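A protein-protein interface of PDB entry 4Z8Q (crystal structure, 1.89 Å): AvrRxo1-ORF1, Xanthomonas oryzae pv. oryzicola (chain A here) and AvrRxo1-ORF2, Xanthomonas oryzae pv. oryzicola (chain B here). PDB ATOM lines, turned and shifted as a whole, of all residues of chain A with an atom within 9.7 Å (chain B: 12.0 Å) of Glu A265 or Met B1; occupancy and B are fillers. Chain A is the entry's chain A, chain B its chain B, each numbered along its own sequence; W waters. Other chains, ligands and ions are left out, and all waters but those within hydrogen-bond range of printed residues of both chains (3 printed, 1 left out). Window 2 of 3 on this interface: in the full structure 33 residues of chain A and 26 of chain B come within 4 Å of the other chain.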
ATOM      1  N   ILE A 228      10.325  -7.250   1.571  1.00  0.00           N
ATOM      2  CA  ILE A 228      11.057  -8.504   1.438  1.00  0.00           C
ATOM      3  C   ILE A 228      10.839  -9.049   0.033  1.00  0.00           C
ATOM      4  O   ILE A 228      11.794  -9.503  -0.606  1.00  0.00           O
ATOM      5  CB  ILE A 228      10.585  -9.531   2.481  1.00  0.00           C
ATOM      6  CG1 ILE A 228      10.939  -9.019   3.872  1.00  0.00           C
ATOM      7  CG2 ILE A 228      11.279 -10.885   2.273  1.00  0.00           C
ATOM      8  CD1 ILE A 228      10.493  -9.917   5.004  1.00  0.00           C
ATOM      9  N   TYR A 240      18.944  -7.774   2.048  1.00  0.00           N
ATOM     10  CA  TYR A 240      17.945  -7.425   3.041  1.00  0.00           C
ATOM     11  C   TYR A 240      18.191  -8.251   4.296  1.00  0.00           C
ATOM     12  O   TYR A 240      18.430  -9.460   4.219  1.00  0.00           O
ATOM     13  CB  TYR A 240      16.539  -7.742   2.496  1.00  0.00           C
ATOM     14  CG  TYR A 240      15.436  -7.590   3.531  1.00  0.00           C
ATOM     15  CD1 TYR A 240      15.099  -8.646   4.383  1.00  0.00           C
ATOM     16  CD2 TYR A 240      14.735  -6.408   3.650  1.00  0.00           C
ATOM     17  CE1 TYR A 240      14.099  -8.514   5.327  1.00  0.00           C
ATOM     18  CE2 TYR A 240      13.729  -6.266   4.600  1.00  0.00           C
ATOM     19  CZ  TYR A 240      13.421  -7.327   5.430  1.00  0.00           C
ATOM     20  OH  TYR A 240      12.414  -7.183   6.363  1.00  0.00           O
ATOM     21  N   ARG A 241      18.125  -7.608   5.458  1.00  0.00           N
ATOM     22  CA  ARG A 241      18.124  -8.334   6.715  1.00  0.00           C
ATOM     23  C   ARG A 241      17.078  -7.740   7.626  1.00  0.00           C
ATOM     24  O   ARG A 241      16.967  -6.521   7.739  1.00  0.00           O
ATOM     25  CB  ARG A 241      19.489  -8.285   7.405  1.00  0.00           C
ATOM     26  CG  ARG A 241      20.576  -9.060   6.690  1.00  0.00           C
ATOM     27  CD  ARG A 241      21.914  -8.842   7.362  1.00  0.00           C
ATOM     28  NE  ARG A 241      22.461  -7.522   7.075  1.00  0.00           N
ATOM     29  CZ  ARG A 241      23.375  -6.913   7.830  1.00  0.00           C
ATOM     30  NH1 ARG A 241      23.821  -7.506   8.926  1.00  0.00           N
ATOM     31  NH2 ARG A 241      23.829  -5.709   7.501  1.00  0.00           N
ATOM     32  N   LEU A 242      16.328  -8.618   8.271  1.00  0.00           N
ATOM     33  CA  LEU A 242      15.294  -8.219   9.200  1.00  0.00           C
ATOM     34  C   LEU A 242      15.713  -8.677  10.587  1.00  0.00           C
ATOM     35  O   LEU A 242      16.036  -9.841  10.765  1.00  0.00           O
ATOM     36  CB  LEU A 242      13.975  -8.889   8.832  1.00  0.00           C
ATOM     37  CG  LEU A 242      12.854  -8.786   9.871  1.00  0.00           C
ATOM     38  CD1 LEU A 242      12.399  -7.336  10.068  1.00  0.00           C
ATOM     39  CD2 LEU A 242      11.691  -9.665   9.409  1.00  0.00           C
ATOM     40  N   PHE A 243      15.723  -7.752  11.547  1.00  0.00           N
ATOM     41  CA  PHE A 243      16.066  -8.062  12.934  1.00  0.00           C
ATOM     42  C   PHE A 243      14.860  -7.781  13.808  1.00  0.00           C
ATOM     43  O   PHE A 243      14.251  -6.713  13.696  1.00  0.00           O
ATOM     44  CB  PHE A 243      17.221  -7.181  13.403  1.00  0.00           C
ATOM     45  CG  PHE A 243      18.511  -7.479  12.727  1.00  0.00           C
ATOM     46  CD1 PHE A 243      19.329  -8.497  13.197  1.00  0.00           C
ATOM     47  CD2 PHE A 243      18.915  -6.742  11.616  1.00  0.00           C
ATOM     48  CE1 PHE A 243      20.532  -8.779  12.577  1.00  0.00           C
ATOM     49  CE2 PHE A 243      20.114  -7.026  10.984  1.00  0.00           C
ATOM     50  CZ  PHE A 243      20.918  -8.047  11.465  1.00  0.00           C
ATOM     51  N   GLY A 244      14.508  -8.742  14.660  1.00  0.00           N
ATOM     52  CA  GLY A 244      13.409  -8.571  15.583  1.00  0.00           C
ATOM     53  C   GLY A 244      13.929  -8.583  17.004  1.00  0.00           C
ATOM     54  O   GLY A 244      15.125  -8.796  17.215  1.00  0.00           O
ATOM     55  N   VAL A 252      17.589 -10.139  17.238  1.00  0.00           N
ATOM     56  CA  VAL A 252      18.004 -11.389  16.600  1.00  0.00           C
ATOM     57  C   VAL A 252      17.592 -11.350  15.129  1.00  0.00           C
ATOM     58  O   VAL A 252      16.611 -10.672  14.770  1.00  0.00           O
ATOM     59  CB  VAL A 252      17.358 -12.626  17.277  1.00  0.00           C
ATOM     60  CG1 VAL A 252      17.804 -12.752  18.740  1.00  0.00           C
ATOM     61  CG2 VAL A 252      15.839 -12.557  17.177  1.00  0.00           C
ATOM     62  N   MET A 253      18.324 -12.037  14.259  1.00  0.00           N
ATOM     63  CA  MET A 253      17.909 -12.007  12.864  1.00  0.00           C
ATOM     64  C   MET A 253      16.724 -12.934  12.699  1.00  0.00           C
ATOM     65  O   MET A 253      16.707 -14.052  13.235  1.00  0.00           O
ATOM     66  CB  MET A 253      19.012 -12.368  11.871  1.00  0.00           C
ATOM     67  CG  MET A 253      18.884 -11.590  10.522  1.00  0.00           C
ATOM     68  SD  MET A 253      20.046 -12.426   9.299  1.00  0.00           S
ATOM     69  CE  MET A 253      21.703 -11.664  10.036  1.00  0.00           C
ATOM     70  N   VAL A 254      15.740 -12.455  11.943  1.00  0.00           N
ATOM     71  CA  VAL A 254      14.481 -13.155  11.757  1.00  0.00           C
ATOM     72  C   VAL A 254      14.338 -13.665  10.322  1.00  0.00           C
ATOM     73  O   VAL A 254      13.939 -14.824  10.094  1.00  0.00           O
ATOM     74  CB  VAL A 254      13.305 -12.221  12.098  1.00  0.00           C
ATOM     75  CG1 VAL A 254      11.968 -12.881  11.734  1.00  0.00           C
ATOM     76  CG2 VAL A 254      13.342 -11.820  13.584  1.00  0.00           C
ATOM     77  N   ALA A 255      14.693 -12.818   9.359  1.00  0.00           N
ATOM     78  CA  ALA A 255      14.673 -13.208   7.954  1.00  0.00           C
ATOM     79  C   ALA A 255      15.710 -12.431   7.169  1.00  0.00           C
ATOM     80  O   ALA A 255      16.109 -11.336   7.575  1.00  0.00           O
ATOM     81  CB  ALA A 255      13.288 -12.968   7.342  1.00  0.00           C
ATOM     82  N   SER A 256      16.115 -12.976   6.029  1.00  0.00           N
ATOM     83  CA  SER A 256      17.152 -12.334   5.235  1.00  0.00           C
ATOM     84  C   SER A 256      17.031 -12.686   3.762  1.00  0.00           C
ATOM     85  O   SER A 256      16.622 -13.783   3.409  1.00  0.00           O
ATOM     86  CB  SER A 256      18.541 -12.742   5.735  1.00  0.00           C
ATOM     87  OG  SER A 256      18.750 -14.133   5.567  1.00  0.00           O
ATOM     88  N   VAL A 257      17.414 -11.747   2.902  1.00  0.00           N
ATOM     89  CA  VAL A 257      17.628 -12.077   1.507  1.00  0.00           C
ATOM     90  C   VAL A 257      19.039 -11.629   1.177  1.00  0.00           C
ATOM     91  O   VAL A 257      19.297 -10.439   1.007  1.00  0.00           O
ATOM     92  CB  VAL A 257      16.616 -11.415   0.576  1.00  0.00           C
ATOM     93  CG1 VAL A 257      16.688 -12.080  -0.825  1.00  0.00           C
ATOM     94  CG2 VAL A 257      15.209 -11.539   1.147  1.00  0.00           C
ATOM     95  N   ILE A 258      19.957 -12.593   1.108  1.00  0.00           N
ATOM     96  CA  ILE A 258      21.374 -12.279   0.964  1.00  0.00           C
ATOM     97  C   ILE A 258      21.934 -13.060  -0.206  1.00  0.00           C
ATOM     98  O   ILE A 258      21.959 -14.293  -0.173  1.00  0.00           O
ATOM     99  CB  ILE A 258      22.176 -12.666   2.213  1.00  0.00           C
ATOM    100  CG1 ILE A 258      21.681 -11.897   3.443  1.00  0.00           C
ATOM    101  CG2 ILE A 258      23.663 -12.351   1.995  1.00  0.00           C
ATOM    102  CD1 ILE A 258      22.232 -12.434   4.764  1.00  0.00           C
ATOM    103  N   GLU A 261      19.343 -15.026  -1.970  1.00  0.00           N
ATOM    104  CA  GLU A 261      18.960 -16.236  -1.272  1.00  0.00           C
ATOM    105  C   GLU A 261      18.104 -15.871  -0.054  1.00  0.00           C
ATOM    106  O   GLU A 261      18.539 -15.116   0.821  1.00  0.00           O
ATOM    107  CB  GLU A 261      20.222 -16.979  -0.862  1.00  0.00           C
ATOM    108  CG  GLU A 261      20.048 -18.422  -0.511  1.00  0.00           C
ATOM    109  CD  GLU A 261      21.253 -19.252  -0.923  1.00  0.00           C
ATOM    110  OE1 GLU A 261      21.732 -19.082  -2.067  1.00  0.00           O
ATOM    111  OE2 GLU A 261      21.722 -20.069  -0.107  1.00  0.00           O
ATOM    112  N   PHE A 262      16.892 -16.412   0.001  1.00  0.00           N
ATOM    113  CA  PHE A 262      15.944 -16.088   1.075  1.00  0.00           C
ATOM    114  C   PHE A 262      15.901 -17.147   2.183  1.00  0.00           C
ATOM    115  O   PHE A 262      15.740 -18.347   1.917  1.00  0.00           O
ATOM    116  CB  PHE A 262      14.555 -15.860   0.490  1.00  0.00           C
ATOM    117  CG  PHE A 262      13.498 -15.641   1.522  1.00  0.00           C
ATOM    118  CD1 PHE A 262      13.512 -14.499   2.325  1.00  0.00           C
ATOM    119  CD2 PHE A 262      12.484 -16.565   1.690  1.00  0.00           C
ATOM    120  CE1 PHE A 262      12.535 -14.292   3.265  1.00  0.00           C
ATOM    121  CE2 PHE A 262      11.509 -16.372   2.642  1.00  0.00           C
ATOM    122  CZ  PHE A 262      11.529 -15.234   3.434  1.00  0.00           C
ATOM    123  N   SER A 263      16.040 -16.695   3.431  1.00  0.00           N
ATOM    124  CA  SER A 263      16.058 -17.598   4.571  1.00  0.00           C
ATOM    125  C   SER A 263      15.242 -17.039   5.718  1.00  0.00           C
ATOM    126  O   SER A 263      15.125 -15.833   5.864  1.00  0.00           O
ATOM    127  CB  SER A 263      17.500 -17.833   5.030  1.00  0.00           C
ATOM    128  OG  SER A 263      18.188 -18.629   4.083  1.00  0.00           O
ATOM    129  N   VAL A 264      14.665 -17.919   6.531  1.00  0.00           N
ATOM    130  CA  VAL A 264      13.924 -17.470   7.702  1.00  0.00           C
ATOM    131  C   VAL A 264      14.574 -17.997   8.984  1.00  0.00           C
ATOM    132  O   VAL A 264      14.349 -19.153   9.387  1.00  0.00           O
ATOM    133  CB  VAL A 264      12.431 -17.884   7.623  1.00  0.00           C
ATOM    134  CG1 VAL A 264      11.690 -17.448   8.883  1.00  0.00           C
ATOM    135  CG2 VAL A 264      11.781 -17.244   6.394  1.00  0.00           C
ATOM    136  N   GLU A 265      15.390 -17.151   9.611  1.00  0.00           N
ATOM    137  CA  GLU A 265      16.168 -17.571  10.781  1.00  0.00           C
ATOM    138  C   GLU A 265      15.323 -17.776  12.028  1.00  0.00           C
ATOM    139  O   GLU A 265      15.684 -18.557  12.915  1.00  0.00           O
ATOM    140  CB  GLU A 265      17.312 -16.597  11.056  1.00  0.00           C
ATOM    141  CG  GLU A 265      18.430 -16.603   9.981  1.00  0.00           C
ATOM    142  CD  GLU A 265      18.093 -15.759   8.770  1.00  0.00           C
ATOM    143  OE1 GLU A 265      18.779 -15.899   7.732  1.00  0.00           O
ATOM    144  OE2 GLU A 265      17.159 -14.929   8.854  1.00  0.00           O
ATOM    145  N   ASN A 266      14.189 -17.088  12.101  1.00  0.00           N
ATOM    146  CA  ASN A 266      13.280 -17.271  13.227  1.00  0.00           C
ATOM    147  C   ASN A 266      11.836 -17.184  12.766  1.00  0.00           C
ATOM    148  O   ASN A 266      11.266 -16.110  12.759  1.00  0.00           O
ATOM    149  CB  ASN A 266      13.560 -16.225  14.323  1.00  0.00           C
ATOM    150  CG  ASN A 266      12.882 -16.559  15.648  1.00  0.00           C
ATOM    151  OD1 ASN A 266      11.689 -16.826  15.694  1.00  0.00           O
ATOM    152  ND2 ASN A 266      13.655 -16.548  16.731  1.00  0.00           N
ATOM    153  N   ALA A 267      11.235 -18.321  12.415  1.00  0.00           N
ATOM    154  CA  ALA A 267       9.904 -18.319  11.831  1.00  0.00           C
ATOM    155  C   ALA A 267       8.811 -17.860  12.790  1.00  0.00           C
ATOM    156  O   ALA A 267       7.827 -17.257  12.364  1.00  0.00           O
ATOM    157  CB  ALA A 267       9.574 -19.700  11.246  1.00  0.00           C
ATOM    158  N   GLU A 268       8.956 -18.169  14.075  1.00  0.00           N
ATOM    159  CA  GLU A 268       8.020 -17.674  15.075  1.00  0.00           C
ATOM    160  C   GLU A 268       7.987 -16.141  15.101  1.00  0.00           C
ATOM    161  O   GLU A 268       6.912 -15.548  15.059  1.00  0.00           O
ATOM    162  CB  GLU A 268       8.334 -18.241  16.475  1.00  0.00           C
ATOM    163  CG  GLU A 268       7.452 -17.650  17.588  1.00  0.00           C
ATOM    164  CD  GLU A 268       7.505 -18.434  18.896  1.00  0.00           C
ATOM    165  OE1 GLU A 268       6.985 -17.915  19.911  1.00  0.00           O
ATOM    166  OE2 GLU A 268       8.051 -19.563  18.913  1.00  0.00           O
ATOM    167  N   LEU A 269       9.147 -15.493  15.170  1.00  0.00           N
ATOM    168  CA  LEU A 269       9.166 -14.031  15.155  1.00  0.00           C
ATOM    169  C   LEU A 269       8.685 -13.492  13.810  1.00  0.00           C
ATOM    170  O   LEU A 269       8.052 -12.436  13.753  1.00  0.00           O
ATOM    171  CB  LEU A 269      10.555 -13.475  15.472  1.00  0.00           C
ATOM    172  CG  LEU A 269      10.835 -13.033  16.907  1.00  0.00           C
ATOM    173  CD1 LEU A 269      12.259 -12.553  16.987  1.00  0.00           C
ATOM    174  CD2 LEU A 269       9.879 -11.920  17.364  1.00  0.00           C
ATOM    175  N   TYR A 270       8.997 -14.203  12.729  1.00  0.00           N
ATOM    176  CA  TYR A 270       8.621 -13.732  11.389  1.00  0.00           C
ATOM    177  C   TYR A 270       7.111 -13.643  11.274  1.00  0.00           C
ATOM    178  O   TYR A 270       6.571 -12.664  10.746  1.00  0.00           O
ATOM    179  CB  TYR A 270       9.188 -14.672  10.325  1.00  0.00           C
ATOM    180  CG  TYR A 270       9.125 -14.143   8.908  1.00  0.00           C
ATOM    181  CD1 TYR A 270       9.448 -12.820   8.613  1.00  0.00           C
ATOM    182  CD2 TYR A 270       8.771 -14.975   7.864  1.00  0.00           C
ATOM    183  CE1 TYR A 270       9.389 -12.344   7.307  1.00  0.00           C
ATOM    184  CE2 TYR A 270       8.727 -14.524   6.572  1.00  0.00           C
ATOM    185  CZ  TYR A 270       9.033 -13.211   6.289  1.00  0.00           C
ATOM    186  OH  TYR A 270       8.978 -12.797   4.969  1.00  0.00           O
ATOM    187  N   GLU A 271       6.417 -14.649  11.788  1.00  0.00           N
ATOM    188  CA  GLU A 271       4.955 -14.609  11.785  1.00  0.00           C
ATOM    189  C   GLU A 271       4.432 -13.427  12.622  1.00  0.00           C
ATOM    190  O   GLU A 271       3.484 -12.734  12.235  1.00  0.00           O
ATOM    191  CB  GLU A 271       4.383 -15.942  12.292  1.00  0.00           C
ATOM    192  CG  GLU A 271       2.861 -15.979  12.329  1.00  0.00           C
ATOM    193  CD  GLU A 271       2.309 -17.382  12.591  1.00  0.00           C
ATOM    194  OE1 GLU A 271       3.121 -18.317  12.704  1.00  0.00           O
ATOM    195  OE2 GLU A 271       1.065 -17.549  12.686  1.00  0.00           O
ATOM    196  N   MET B   1      15.973 -21.575  16.957  1.00  0.00           N
ATOM    197  CA  MET B   1      15.376 -22.698  16.240  1.00  0.00           C
ATOM    198  C   MET B   1      16.023 -22.849  14.867  1.00  0.00           C
ATOM    199  O   MET B   1      16.789 -21.980  14.433  1.00  0.00           O
ATOM    200  CB  MET B   1      13.864 -22.500  16.092  1.00  0.00           C
ATOM    201  CG  MET B   1      13.465 -21.455  15.048  1.00  0.00           C
ATOM    202  SD  MET B   1      11.768 -20.547  15.412  1.00  0.00           S
ATOM    203  CE  MET B   1      10.512 -21.906  14.898  1.00  0.00           C
ATOM    204  N   LYS B   2      15.709 -23.949  14.190  1.00  0.00           N
ATOM    205  CA  LYS B   2      16.226 -24.207  12.851  1.00  0.00           C
ATOM    206  C   LYS B   2      15.782 -23.128  11.877  1.00  0.00           C
ATOM    207  O   LYS B   2      14.628 -22.678  11.882  1.00  0.00           O
ATOM    208  CB  LYS B   2      15.807 -25.604  12.366  1.00  0.00           C
ATOM    209  CG  LYS B   2      16.098 -25.929  10.887  1.00  0.00           C
ATOM    210  CD  LYS B   2      17.580 -25.836  10.532  1.00  0.00           C
ATOM    211  CE  LYS B   2      17.795 -25.970   9.017  1.00  0.00           C
ATOM    212  NZ  LYS B   2      18.718 -24.903   8.487  1.00  0.00           N
ATOM    213  N   THR B   3      16.732 -22.685  11.070  1.00  0.00           N
ATOM    214  CA  THR B   3      16.483 -21.701  10.039  1.00  0.00           C
ATOM    215  C   THR B   3      15.740 -22.363   8.883  1.00  0.00           C
ATOM    216  O   THR B   3      16.121 -23.446   8.425  1.00  0.00           O
ATOM    217  CB  THR B   3      17.816 -21.121   9.554  1.00  0.00           C
ATOM    218  OG1 THR B   3      18.393 -20.360  10.624  1.00  0.00           O
ATOM    219  CG2 THR B   3      17.623 -20.229   8.343  1.00  0.00           C
ATOM    220  N   LEU B   4      14.665 -21.745   8.416  1.00  0.00           N
ATOM    221  CA  LEU B   4      14.007 -22.261   7.211  1.00  0.00           C
ATOM    222  C   LEU B   4      14.781 -21.773   5.988  1.00  0.00           C
ATOM    223  O   LEU B   4      15.138 -20.590   5.898  1.00  0.00           O
ATOM    224  CB  LEU B   4      12.548 -21.794   7.136  1.00  0.00           C
ATOM    225  CG  LEU B   4      11.643 -21.958   8.362  1.00  0.00           C
ATOM    226  CD1 LEU B   4      10.239 -21.487   8.032  1.00  0.00           C
ATOM    227  CD2 LEU B   4      11.592 -23.384   8.828  1.00  0.00           C
ATOM    228  N   THR B   5      15.035 -22.678   5.041  1.00  0.00           N
ATOM    229  CA  THR B   5      15.806 -22.354   3.844  1.00  0.00           C
ATOM    230  C   THR B   5      15.093 -22.860   2.596  1.00  0.00           C
ATOM    231  O   THR B   5      14.111 -23.614   2.688  1.00  0.00           O
ATOM    232  CB  THR B   5      17.211 -23.020   3.862  1.00  0.00           C
ATOM    233  OG1 THR B   5      17.054 -24.434   3.704  1.00  0.00           O
ATOM    234  CG2 THR B   5      17.945 -22.748   5.175  1.00  0.00           C
ATOM    235  N   GLY B   6      15.592 -22.447   1.435  1.00  0.00           N
ATOM    236  CA  GLY B   6      15.114 -22.962   0.155  1.00  0.00           C
ATOM    237  C   GLY B   6      13.603 -23.000  -0.001  1.00  0.00           C
ATOM    238  O   GLY B   6      12.909 -22.016   0.280  1.00  0.00           O
ATOM    239  N   ASP B   8      11.296 -24.521   1.677  1.00  0.00           N
ATOM    240  CA  ASP B   8      10.496 -24.349   2.888  1.00  0.00           C
ATOM    241  C   ASP B   8      10.370 -22.878   3.272  1.00  0.00           C
ATOM    242  O   ASP B   8       9.295 -22.423   3.661  1.00  0.00           O
ATOM    243  CB  ASP B   8      11.056 -25.163   4.058  1.00  0.00           C
ATOM    244  CG  ASP B   8      10.735 -26.653   3.947  1.00  0.00           C
ATOM    245  OD1 ASP B   8       9.976 -27.046   3.039  1.00  0.00           O
ATOM    246  OD2 ASP B   8      11.239 -27.427   4.783  1.00  0.00           O
ATOM    247  N   ALA B   9      11.468 -22.133   3.172  1.00  0.00           N
ATOM    248  CA  ALA B   9      11.433 -20.714   3.497  1.00  0.00           C
ATOM    249  C   ALA B   9      10.441 -20.024   2.572  1.00  0.00           C
ATOM    250  O   ALA B   9       9.588 -19.259   3.013  1.00  0.00           O
ATOM    251  CB  ALA B   9      12.826 -20.087   3.353  1.00  0.00           C
ATOM    252  N   LEU B  10      10.560 -20.284   1.278  1.00  0.00           N
ATOM    253  CA  LEU B  10       9.666 -19.649   0.309  1.00  0.00           C
ATOM    254  C   LEU B  10       8.213 -20.001   0.565  1.00  0.00           C
ATOM    255  O   LEU B  10       7.350 -19.150   0.448  1.00  0.00           O
ATOM    256  CB  LEU B  10      10.046 -20.030  -1.131  1.00  0.00           C
ATOM    257  CG  LEU B  10      11.266 -19.341  -1.726  1.00  0.00           C
ATOM    258  CD1 LEU B  10      11.626 -19.976  -3.090  1.00  0.00           C
ATOM    259  CD2 LEU B  10      11.008 -17.861  -1.889  1.00  0.00           C
ATOM    260  N   PHE B  12       6.868 -20.944   3.488  1.00  0.00           N
ATOM    261  CA  PHE B  12       6.434 -20.299   4.736  1.00  0.00           C
ATOM    262  C   PHE B  12       6.053 -18.865   4.454  1.00  0.00           C
ATOM    263  O   PHE B  12       5.055 -18.364   4.969  1.00  0.00           O
ATOM    264  CB  PHE B  12       7.544 -20.308   5.780  1.00  0.00           C
ATOM    265  CG  PHE B  12       7.059 -20.012   7.189  1.00  0.00           C
ATOM    266  CD1 PHE B  12       6.509 -21.023   7.967  1.00  0.00           C
ATOM    267  CD2 PHE B  12       7.174 -18.742   7.734  1.00  0.00           C
ATOM    268  CE1 PHE B  12       6.072 -20.771   9.272  1.00  0.00           C
ATOM    269  CE2 PHE B  12       6.726 -18.481   9.039  1.00  0.00           C
ATOM    270  CZ  PHE B  12       6.184 -19.507   9.799  1.00  0.00           C
ATOM    271  N   HIS B  13       6.876 -18.203   3.647  1.00  0.00           N
ATOM    272  CA  HIS B  13       6.666 -16.813   3.263  1.00  0.00           C
ATOM    273  C   HIS B  13       5.349 -16.676   2.475  1.00  0.00           C
ATOM    274  O   HIS B  13       4.533 -15.790   2.742  1.00  0.00           O
ATOM    275  CB  HIS B  13       7.881 -16.354   2.441  1.00  0.00           C
ATOM    276  CG  HIS B  13       7.799 -14.949   1.933  1.00  0.00           C
ATOM    277  ND1 HIS B  13       8.121 -13.848   2.706  1.00  0.00           N
ATOM    278  CD2 HIS B  13       7.462 -14.467   0.717  1.00  0.00           C
ATOM    279  CE1 HIS B  13       7.954 -12.752   1.988  1.00  0.00           C
ATOM    280  NE2 HIS B  13       7.552 -13.099   0.779  1.00  0.00           N
ATOM    281  N   LEU B  16       2.390 -17.213   4.825  1.00  0.00           N
ATOM    282  CA  LEU B  16       2.281 -16.139   5.789  1.00  0.00           C
ATOM    283  C   LEU B  16       1.726 -14.890   5.109  1.00  0.00           C
ATOM    284  O   LEU B  16       0.954 -14.165   5.700  1.00  0.00           O
ATOM    285  CB  LEU B  16       3.644 -15.862   6.439  1.00  0.00           C
ATOM    286  CG  LEU B  16       3.686 -14.781   7.497  1.00  0.00           C
ATOM    287  CD1 LEU B  16       2.699 -15.101   8.637  1.00  0.00           C
ATOM    288  CD2 LEU B  16       5.119 -14.619   8.025  1.00  0.00           C
HETATM  289  O   HOH W   1      14.378 -19.530  -0.231  1.00  0.00           O
HETATM  290  O   HOH W   2      17.928 -20.062  13.371  1.00  0.00           O
HETATM  291  O   HOH W   3      17.632 -20.360   1.527  1.00  0.00           O
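Glu A265 touches just these residues of chain B: Met B1 (3.9 Å) and Thr B3 (3.6 Å). Met B1 touches four residues of chain A. No residue of chain B comes within 4 Å of Met A253. No residue of chain B comes within 4 Å of Val A254. No residue of chain B comes within 4 Å of Ala A255. No residue of chain B comes within 4 Å of Ser A256. Of chain B, only Leu B4 (3.4 Å) comes within 4 Å of Ser A263. Val A264 touches two residues of chain B. Of chain B, only Met B1 (3.9 Å) comes within 4 Å of Glu A268. Of the printed residues of chain A, Phe B12 touches Ala A267 (3.7 Å). Printed residues of chain B within 4 Å of Phe A262: Ala B9 and His B13. Printed residues of chain A within 4 Å of Thr B3: Val A264 and Glu A265. Printed residues of chain A within 4 Å of Ala B9: Phe A262. Gly A244 touches none of the printed residues of chain B. The nearest residue of chain B that does not touch Glu A265 is Lys B2 (4.4 Å). The nearest printed residue of chain B that does not touch Glu A271 is Phe B12 (4.4 Å).
Water W2 lies within hydrogen-bond range of the backbone carbonyl oxygen (O) of Met B1, the backbone carbonyl oxygen (O) of Glu A265 and the side-chain hydroxyl (OG1) of Thr B3. Water W3 lies within hydrogen-bond range of the backbone carbonyl oxygen of Phe A262 (2.8 Å), the backbone NH of Gly B6 (2.9 Å) and the side-chain hydroxyl of Ser A263 (3.1 Å). Water W1 bridges the backbone carbonyl oxygen of Phe A262 (2.8 Å) and the backbone carbonyl oxygen of Gly B6 (2.9 Å).
The side-chain amide oxygen (OD1) of Asn A266 sits at hydrogen-bond distance from the backbone NH (N) of Leu A269, at 2.9 Å. The backbone NH (N) of Ser A263 lies within hydrogen-bond range of the backbone carbonyl oxygen (O) of Ser A256 (3.0 Å). The backbone carbonyl oxygen (O) of Val A254 sits at hydrogen-bond distance from the backbone NH (N) of Glu A265, at 2.8 Å. The backbone NH (N) of Ala A255 lies close to the side-chain carboxylate (OE2) of Glu A265, at 3.3 Å. The backbone NH of Glu A268 sits close to the side-chain amide oxygen of Asn A266 (3.4 Å). The backbone NH (N) of Asn A266 sits at hydrogen-bond distance from the backbone carbonyl oxygen (O) of Val A254 (3.0 Å).
Of the 12 printed residues of chain B, 7 touch a printed residue of chain A. Hydrophobic or aromatic side chains of chain B that line the printed part of chain A: Met B1, Leu B4, Ala B9, Phe B12, His B13 and Leu B16. Of the 24 printed residues of chain A, 10 touch a printed residue of chain B. Along chain A the printed residues that touch a printed residue of chain B span positions 228 to 271. Among the printed residues, 16 pairs touch across the chains.
The side-chain amide oxygen of Asn A266 sits close to the side-chain sulfur of Met B1, 3.7 Å away. The side-chain hydroxyl (OH) of Tyr A270 lies within hydrogen-bond range of a ring nitrogen (ND1) of His B13, at 2.6 Å. The backbone NH of Val A264 is in hydrogen-bond range of the backbone carbonyl oxygen of Leu B4 (2.8 Å). SD of Met B1 lies within hydrogen-bond range of N of Ala A267 (3.8 Å).
Among the printed residues, merely in contact across the chains: Val A264 with Thr B3 (3.4 Å), Ser A263 with Leu B4 (3.4 Å), Phe A262 with Ala B9 (3.5 Å), Glu A265 with Thr B3 (3.6 Å), Phe A262 with His B13 (3.6 Å), Tyr A270 with Leu B16 (3.7 Å), Ala A267 with Phe B12 (3.7 Å), Ala A267 with Leu B4 (3.7 Å), Glu A271 with Leu B16 (3.8 Å), Ile A228 with His B13 (3.8 Å), Glu A265 with Met B1 (3.9 Å) and Glu A268 with Met B1 (3.9 Å).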
